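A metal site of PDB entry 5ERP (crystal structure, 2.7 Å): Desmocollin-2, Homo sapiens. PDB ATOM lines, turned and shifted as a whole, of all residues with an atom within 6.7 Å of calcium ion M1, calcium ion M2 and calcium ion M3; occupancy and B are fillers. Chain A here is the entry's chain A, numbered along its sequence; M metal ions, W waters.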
ATOM      1  N   GLU A 247     -23.303   9.397  22.727  1.00  0.00           N
ATOM      2  CA  GLU A 247     -22.209   8.469  22.988  1.00  0.00           C
ATOM      3  C   GLU A 247     -22.504   7.537  24.159  1.00  0.00           C
ATOM      4  O   GLU A 247     -22.050   6.399  24.186  1.00  0.00           O
ATOM      5  CB  GLU A 247     -20.933   9.273  23.275  1.00  0.00           C
ATOM      6  CG  GLU A 247     -19.794   8.492  23.905  1.00  0.00           C
ATOM      7  CD  GLU A 247     -18.691   9.392  24.427  1.00  0.00           C
ATOM      8  OE1 GLU A 247     -18.717  10.608  24.120  1.00  0.00           O
ATOM      9  OE2 GLU A 247     -17.813   8.888  25.150  1.00  0.00           O
ATOM     10  N   LEU A 298     -21.443   2.571  23.100  1.00  0.00           N
ATOM     11  CA  LEU A 298     -20.626   3.329  22.164  1.00  0.00           C
ATOM     12  C   LEU A 298     -19.533   4.078  22.920  1.00  0.00           C
ATOM     13  O   LEU A 298     -19.614   4.268  24.134  1.00  0.00           O
ATOM     14  CB  LEU A 298     -21.494   4.308  21.366  1.00  0.00           C
ATOM     15  CG  LEU A 298     -22.804   3.730  20.813  1.00  0.00           C
ATOM     16  CD1 LEU A 298     -23.594   4.789  20.054  1.00  0.00           C
ATOM     17  CD2 LEU A 298     -22.545   2.515  19.935  1.00  0.00           C
ATOM     18  N   ASP A 299     -18.510   4.510  22.186  1.00  0.00           N
ATOM     19  CA  ASP A 299     -17.410   5.280  22.746  1.00  0.00           C
ATOM     20  C   ASP A 299     -16.840   6.197  21.681  1.00  0.00           C
ATOM     21  O   ASP A 299     -16.187   5.747  20.744  1.00  0.00           O
ATOM     22  CB  ASP A 299     -16.318   4.354  23.291  1.00  0.00           C
ATOM     23  CG  ASP A 299     -15.148   5.113  23.888  1.00  0.00           C
ATOM     24  OD1 ASP A 299     -15.337   6.274  24.315  1.00  0.00           O
ATOM     25  OD2 ASP A 299     -14.035   4.557  23.909  1.00  0.00           O
ATOM     26  N   ARG A 300     -17.092   7.500  21.815  1.00  0.00           N
ATOM     27  CA  ARG A 300     -16.604   8.472  20.847  1.00  0.00           C
ATOM     28  C   ARG A 300     -15.086   8.493  20.813  1.00  0.00           C
ATOM     29  O   ARG A 300     -14.484   8.768  19.777  1.00  0.00           O
ATOM     30  CB  ARG A 300     -17.153   9.869  21.162  1.00  0.00           C
ATOM     31  CG  ARG A 300     -16.631  10.971  20.254  1.00  0.00           C
ATOM     32  CD  ARG A 300     -17.120  12.331  20.683  1.00  0.00           C
ATOM     33  NE  ARG A 300     -16.336  13.416  20.090  1.00  0.00           N
ATOM     34  CZ  ARG A 300     -15.133  13.791  20.507  1.00  0.00           C
ATOM     35  NH1 ARG A 300     -14.553  13.175  21.531  1.00  0.00           N
ATOM     36  NH2 ARG A 300     -14.506  14.789  19.894  1.00  0.00           N
ATOM     37  N   GLU A 301     -14.468   8.173  21.943  1.00  0.00           N
ATOM     38  CA  GLU A 301     -13.021   8.306  22.087  1.00  0.00           C
ATOM     39  C   GLU A 301     -12.261   7.009  21.809  1.00  0.00           C
ATOM     40  O   GLU A 301     -11.056   6.940  22.025  1.00  0.00           O
ATOM     41  CB  GLU A 301     -12.693   8.797  23.502  1.00  0.00           C
ATOM     42  CG  GLU A 301     -13.281  10.164  23.809  1.00  0.00           C
ATOM     43  CD  GLU A 301     -14.749  10.099  24.179  1.00  0.00           C
ATOM     44  OE1 GLU A 301     -15.178   9.069  24.750  1.00  0.00           O
ATOM     45  OE2 GLU A 301     -15.470  11.070  23.897  1.00  0.00           O
ATOM     46  N   ALA A 302     -12.972   5.982  21.341  1.00  0.00           N
ATOM     47  CA  ALA A 302     -12.339   4.720  20.982  1.00  0.00           C
ATOM     48  C   ALA A 302     -11.358   4.930  19.834  1.00  0.00           C
ATOM     49  O   ALA A 302     -11.498   5.893  19.065  1.00  0.00           O
ATOM     50  CB  ALA A 302     -13.382   3.681  20.612  1.00  0.00           C
ATOM     51  N   GLN A 333     -22.393  11.978  19.469  1.00  0.00           N
ATOM     52  CA  GLN A 333     -22.395  13.270  20.139  1.00  0.00           C
ATOM     53  C   GLN A 333     -21.672  13.085  21.461  1.00  0.00           C
ATOM     54  O   GLN A 333     -22.025  12.208  22.256  1.00  0.00           O
ATOM     55  CB  GLN A 333     -23.820  13.794  20.333  1.00  0.00           C
ATOM     56  CG  GLN A 333     -23.886  15.203  20.891  1.00  0.00           C
ATOM     57  CD  GLN A 333     -25.305  15.686  21.095  1.00  0.00           C
ATOM     58  OE1 GLN A 333     -26.258  15.064  20.626  1.00  0.00           O
ATOM     59  NE2 GLN A 333     -25.450  16.829  21.755  1.00  0.00           N
ATOM     60  N   ASP A 334     -20.657  13.904  21.700  1.00  0.00           N
ATOM     61  CA  ASP A 334     -19.793  13.721  22.850  1.00  0.00           C
ATOM     62  C   ASP A 334     -20.482  13.982  24.186  1.00  0.00           C
ATOM     63  O   ASP A 334     -21.359  14.831  24.290  1.00  0.00           O
ATOM     64  CB  ASP A 334     -18.562  14.619  22.762  1.00  0.00           C
ATOM     65  CG  ASP A 334     -17.578  14.373  23.882  1.00  0.00           C
ATOM     66  OD1 ASP A 334     -17.190  13.210  24.091  1.00  0.00           O
ATOM     67  OD2 ASP A 334     -17.216  15.343  24.578  1.00  0.00           O
ATOM     68  N   VAL A 335     -20.057  13.212  25.185  1.00  0.00           N
ATOM     69  CA  VAL A 335     -20.492  13.401  26.554  1.00  0.00           C
ATOM     70  C   VAL A 335     -19.214  13.478  27.395  1.00  0.00           C
ATOM     71  O   VAL A 335     -18.340  12.623  27.267  1.00  0.00           O
ATOM     72  CB  VAL A 335     -21.381  12.230  27.036  1.00  0.00           C
ATOM     73  CG1 VAL A 335     -21.745  12.371  28.499  1.00  0.00           C
ATOM     74  CG2 VAL A 335     -22.642  12.135  26.172  1.00  0.00           C
ATOM     75  N   ASN A 336     -19.098  14.506  28.239  1.00  0.00           N
ATOM     76  CA  ASN A 336     -17.890  14.669  29.027  1.00  0.00           C
ATOM     77  C   ASN A 336     -17.761  13.535  30.040  1.00  0.00           C
ATOM     78  O   ASN A 336     -18.216  13.637  31.180  1.00  0.00           O
ATOM     79  CB  ASN A 336     -17.863  16.021  29.746  1.00  0.00           C
ATOM     80  CG  ASN A 336     -16.476  16.380  30.254  1.00  0.00           C
ATOM     81  OD1 ASN A 336     -15.664  15.508  30.556  1.00  0.00           O
ATOM     82  ND2 ASN A 336     -16.197  17.673  30.356  1.00  0.00           N
ATOM     83  N   ASP A 337     -17.118  12.454  29.604  1.00  0.00           N
ATOM     84  CA  ASP A 337     -16.943  11.260  30.428  1.00  0.00           C
ATOM     85  C   ASP A 337     -15.475  10.861  30.486  1.00  0.00           C
ATOM     86  O   ASP A 337     -15.156   9.715  30.808  1.00  0.00           O
ATOM     87  CB  ASP A 337     -17.790  10.115  29.891  1.00  0.00           C
ATOM     88  CG  ASP A 337     -17.435   9.729  28.457  1.00  0.00           C
ATOM     89  OD1 ASP A 337     -16.576  10.411  27.849  1.00  0.00           O
ATOM     90  OD2 ASP A 337     -18.009   8.743  27.948  1.00  0.00           O
ATOM     91  N   ASN A 338     -14.591  11.796  30.154  1.00  0.00           N
ATOM     92  CA  ASN A 338     -13.160  11.532  30.181  1.00  0.00           C
ATOM     93  C   ASN A 338     -12.364  12.637  30.865  1.00  0.00           C
ATOM     94  O   ASN A 338     -12.577  13.827  30.626  1.00  0.00           O
ATOM     95  CB  ASN A 338     -12.632  11.336  28.756  1.00  0.00           C
ATOM     96  CG  ASN A 338     -13.075  10.015  28.153  1.00  0.00           C
ATOM     97  OD1 ASN A 338     -13.590   9.972  27.037  1.00  0.00           O
ATOM     98  ND2 ASN A 338     -12.895   8.933  28.889  1.00  0.00           N
ATOM     99  N   SER A 339     -11.443  12.224  31.725  1.00  0.00           N
ATOM    100  CA  SER A 339     -10.521  13.116  32.416  1.00  0.00           C
ATOM    101  C   SER A 339      -9.272  13.345  31.578  1.00  0.00           C
ATOM    102  O   SER A 339      -9.029  12.614  30.617  1.00  0.00           O
ATOM    103  CB  SER A 339     -10.146  12.537  33.783  1.00  0.00           C
ATOM    104  OG  SER A 339      -9.824  11.161  33.668  1.00  0.00           O
ATOM    105  N   PRO A 340      -8.477  14.370  31.927  1.00  0.00           N
ATOM    106  CA  PRO A 340      -7.219  14.613  31.204  1.00  0.00           C
ATOM    107  C   PRO A 340      -6.257  13.429  31.303  1.00  0.00           C
ATOM    108  O   PRO A 340      -6.495  12.506  32.080  1.00  0.00           O
ATOM    109  CB  PRO A 340      -6.632  15.842  31.921  1.00  0.00           C
ATOM    110  CG  PRO A 340      -7.810  16.508  32.552  1.00  0.00           C
ATOM    111  CD  PRO A 340      -8.756  15.414  32.931  1.00  0.00           C
ATOM    112  N   ASP A 363      -7.195  15.955  26.606  1.00  0.00           N
ATOM    113  CA  ASP A 363      -8.532  15.489  26.938  1.00  0.00           C
ATOM    114  C   ASP A 363      -9.187  14.888  25.695  1.00  0.00           C
ATOM    115  O   ASP A 363      -9.431  15.595  24.723  1.00  0.00           O
ATOM    116  CB  ASP A 363      -9.382  16.628  27.499  1.00  0.00           C
ATOM    117  CG  ASP A 363     -10.540  16.127  28.342  1.00  0.00           C
ATOM    118  OD1 ASP A 363     -11.195  15.138  27.935  1.00  0.00           O
ATOM    119  OD2 ASP A 363     -10.785  16.708  29.418  1.00  0.00           O
ATOM    120  N   PRO A 364      -9.469  13.565  25.719  1.00  0.00           N
ATOM    121  CA  PRO A 364     -10.078  12.882  24.565  1.00  0.00           C
ATOM    122  C   PRO A 364     -11.398  13.500  24.105  1.00  0.00           C
ATOM    123  O   PRO A 364     -11.740  13.410  22.932  1.00  0.00           O
ATOM    124  CB  PRO A 364     -10.299  11.468  25.089  1.00  0.00           C
ATOM    125  CG  PRO A 364      -9.275  11.281  26.121  1.00  0.00           C
ATOM    126  CD  PRO A 364      -9.147  12.615  26.796  1.00  0.00           C
ATOM    127  N   ASP A 365     -12.131  14.120  25.037  1.00  0.00           N
ATOM    128  CA  ASP A 365     -13.423  14.707  24.705  1.00  0.00           C
ATOM    129  C   ASP A 365     -13.260  15.916  23.791  1.00  0.00           C
ATOM    130  O   ASP A 365     -12.147  16.336  23.499  1.00  0.00           O
ATOM    131  CB  ASP A 365     -14.160  15.117  25.987  1.00  0.00           C
ATOM    132  CG  ASP A 365     -14.425  13.940  26.913  1.00  0.00           C
ATOM    133  OD1 ASP A 365     -14.691  12.831  26.406  1.00  0.00           O
ATOM    134  OD2 ASP A 365     -14.369  14.132  28.141  1.00  0.00           O
ATOM    135  N   GLU A 366     -14.386  16.458  23.352  1.00  0.00           N
ATOM    136  CA  GLU A 366     -14.384  17.622  22.474  1.00  0.00           C
ATOM    137  C   GLU A 366     -13.903  18.862  23.242  1.00  0.00           C
ATOM    138  O   GLU A 366     -13.930  18.867  24.476  1.00  0.00           O
ATOM    139  CB  GLU A 366     -15.784  17.821  21.881  1.00  0.00           C
ATOM    140  CG  GLU A 366     -16.870  18.151  22.893  1.00  0.00           C
ATOM    141  CD  GLU A 366     -18.253  18.135  22.281  1.00  0.00           C
ATOM    142  OE1 GLU A 366     -18.359  18.255  21.037  1.00  0.00           O
ATOM    143  OE2 GLU A 366     -19.243  17.991  23.032  1.00  0.00           O
ATOM    144  N   HIS A 369     -15.419  20.238  26.282  1.00  0.00           N
ATOM    145  CA  HIS A 369     -15.328  19.345  27.437  1.00  0.00           C
ATOM    146  C   HIS A 369     -13.882  18.983  27.753  1.00  0.00           C
ATOM    147  O   HIS A 369     -13.579  17.851  28.142  1.00  0.00           O
ATOM    148  CB  HIS A 369     -16.141  18.082  27.180  1.00  0.00           C
ATOM    149  CG  HIS A 369     -17.615  18.314  27.106  1.00  0.00           C
ATOM    150  ND1 HIS A 369     -18.480  17.436  26.498  1.00  0.00           N
ATOM    151  CD2 HIS A 369     -18.375  19.333  27.574  1.00  0.00           C
ATOM    152  CE1 HIS A 369     -19.720  17.903  26.586  1.00  0.00           C
ATOM    153  NE2 HIS A 369     -19.689  19.049  27.239  1.00  0.00           N
ATOM    154  N   GLY A 370     -12.974  19.953  27.584  1.00  0.00           N
ATOM    155  CA  GLY A 370     -11.560  19.732  27.834  1.00  0.00           C
ATOM    156  C   GLY A 370     -10.904  20.927  28.515  1.00  0.00           C
ATOM    157  O   GLY A 370     -11.204  21.216  29.667  1.00  0.00           O
ATOM    158  N   PHE A 373      -6.942  23.327  31.398  1.00  0.00           N
ATOM    159  CA  PHE A 373      -6.640  22.359  32.444  1.00  0.00           C
ATOM    160  C   PHE A 373      -6.036  23.022  33.668  1.00  0.00           C
ATOM    161  O   PHE A 373      -5.298  24.001  33.552  1.00  0.00           O
ATOM    162  CB  PHE A 373      -5.683  21.288  31.913  1.00  0.00           C
ATOM    163  CG  PHE A 373      -6.189  20.563  30.707  1.00  0.00           C
ATOM    164  CD1 PHE A 373      -7.526  20.257  30.570  1.00  0.00           C
ATOM    165  CD2 PHE A 373      -5.308  20.190  29.702  1.00  0.00           C
ATOM    166  CE1 PHE A 373      -7.993  19.587  29.448  1.00  0.00           C
ATOM    167  CE2 PHE A 373      -5.763  19.530  28.580  1.00  0.00           C
ATOM    168  CZ  PHE A 373      -7.105  19.226  28.460  1.00  0.00           C
ATOM    169  N   ASP A 419      -9.940  18.979  34.293  1.00  0.00           N
ATOM    170  CA  ASP A 419     -10.402  19.719  33.128  1.00  0.00           C
ATOM    171  C   ASP A 419     -11.212  20.944  33.536  1.00  0.00           C
ATOM    172  O   ASP A 419     -11.270  21.297  34.710  1.00  0.00           O
ATOM    173  CB  ASP A 419     -11.228  18.810  32.215  1.00  0.00           C
ATOM    174  CG  ASP A 419     -12.475  18.273  32.898  1.00  0.00           C
ATOM    175  OD1 ASP A 419     -12.609  18.438  34.128  1.00  0.00           O
ATOM    176  OD2 ASP A 419     -13.327  17.684  32.198  1.00  0.00           O
ATOM    177  N   ARG A 420     -11.826  21.586  32.548  1.00  0.00           N
ATOM    178  CA  ARG A 420     -12.627  22.784  32.775  1.00  0.00           C
ATOM    179  C   ARG A 420     -13.767  22.543  33.770  1.00  0.00           C
ATOM    180  O   ARG A 420     -14.158  23.457  34.489  1.00  0.00           O
ATOM    181  CB  ARG A 420     -13.200  23.285  31.450  1.00  0.00           C
ATOM    182  CG  ARG A 420     -13.697  24.719  31.492  1.00  0.00           C
ATOM    183  CD  ARG A 420     -14.251  25.135  30.140  1.00  0.00           C
ATOM    184  NE  ARG A 420     -15.432  24.355  29.798  1.00  0.00           N
ATOM    185  CZ  ARG A 420     -16.667  24.649  30.201  1.00  0.00           C
ATOM    186  NH1 ARG A 420     -16.892  25.702  30.968  1.00  0.00           N
ATOM    187  NH2 ARG A 420     -17.688  23.879  29.836  1.00  0.00           N
ATOM    188  N   MET A 423     -13.360  16.972  35.933  1.00  0.00           N
ATOM    189  CA  MET A 423     -12.999  15.564  35.780  1.00  0.00           C
ATOM    190  C   MET A 423     -11.502  15.443  36.030  1.00  0.00           C
ATOM    191  O   MET A 423     -10.694  15.958  35.250  1.00  0.00           O
ATOM    192  CB  MET A 423     -13.363  15.025  34.401  1.00  0.00           C
ATOM    193  CG  MET A 423     -14.843  14.728  34.210  1.00  0.00           C
ATOM    194  SD  MET A 423     -15.390  13.289  35.168  1.00  0.00           S
ATOM    195  CE  MET A 423     -14.472  11.958  34.378  1.00  0.00           C
HETATM  196 CA    CA M   1     -16.434   7.225  26.271  1.00  0.00          CA
HETATM  197 CA    CA M   2     -16.742  11.602  25.750  1.00  0.00          CA
HETATM  198 CA    CA M   3     -13.330  16.012  29.606  1.00  0.00          CA
HETATM  199  O   HOH W   1     -17.734   4.913  26.448  1.00  0.00           O
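The side-chain carboxylate of Glu 301 lies close to the side-chain amide oxygen of Asn 338. The side-chain carboxylate of Glu 301 lies close to the guanidinium group of Arg 300, 3.3 Å away. The side-chain carboxylate (OD2) of Asp 334 lies within hydrogen-bond range of a ring nitrogen (ND1) of His 369. NH1 of Arg 300 lies close to OD1 of Asp 334, 3.7 Å away. The side-chain carboxylate (OD2) of Asp 334 lies within hydrogen-bond range of the backbone NH (N) of Glu 366, at 3.3 Å. The side-chain carboxylate of Asp 337 sits close to the side-chain amide oxygen of Asn 338, 3.1 Å away. The backbone carbonyl oxygen (O) of Gln 333 sits at hydrogen-bond distance from the backbone NH (N) of Glu 247, 3.1 Å away. The side-chain amide nitrogen (ND2) of Asn 336 sits at hydrogen-bond distance from the side-chain carboxylate (OD2) of Asp 419.
Four residues have an atom within 4 Å of calcium ion M1: Glu 247, Asp 299, Glu 301 and Asp 337. The nearest printed residue that does not touch calcium ion M1 is Asn 338 (4.03 Å).
Of the 24 residues printed, 7 come within 4 Å of calcium ion M2. Along chain A the residues within 4 Å of calcium ion M2 span positions 247 to 365.
Calcium ion M1 is bound by OE2 of Glu 247. OD1 of Asp 299 binds calcium ion M1, at 2.4 Å. Water W1 is bound to calcium ion M1 (2.7 Å). OE1 of Glu 301 binds calcium ion M1 (2.7 Å). Calcium ion M1 is bound by OD2 of Asp 337, 2.8 Å away. Calcium ion M1 has five donor atoms within binding distance.
Calcium ion M2 is bound by OE2 of Glu 301 (2.3 Å), OD1 of Asp 334 (2.4 Å), OD1 of Asp 337 (2.4 Å), O of Val 335 (2.4 Å), OD1 of Asp 365 (2.5 Å) and OE1 of Glu 247 (2.7 Å). Slightly farther from calcium ion M2 lies the side-chain carboxylate (OE2) of Glu 247 (3.0 Å). Slightly farther from calcium ion M2 lies the side-chain carboxylate (OE1) of Glu 301 (3.1 Å).
The backbone carbonyl oxygen (O) of His 369 is bound to calcium ion M3 (2.4 Å). Calcium ion M3 is bound by the backbone carbonyl oxygen (O) of Asn 338 (2.5 Å). The side-chain amide oxygen (OD1) of Asn 336 binds calcium ion M3 (2.6 Å). OD2 of Asp 365 binds calcium ion M3. Calcium ion M3 is bound by the side-chain carboxylate (OD2) of Asp 363, 2.6 Å away. Calcium ion M3 is bound by the side-chain carboxylate (OD1) of Asp 363. Slightly farther from calcium ion M3 lies the side-chain carboxylate (OD2) of Asp 419 (3.1 Å).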
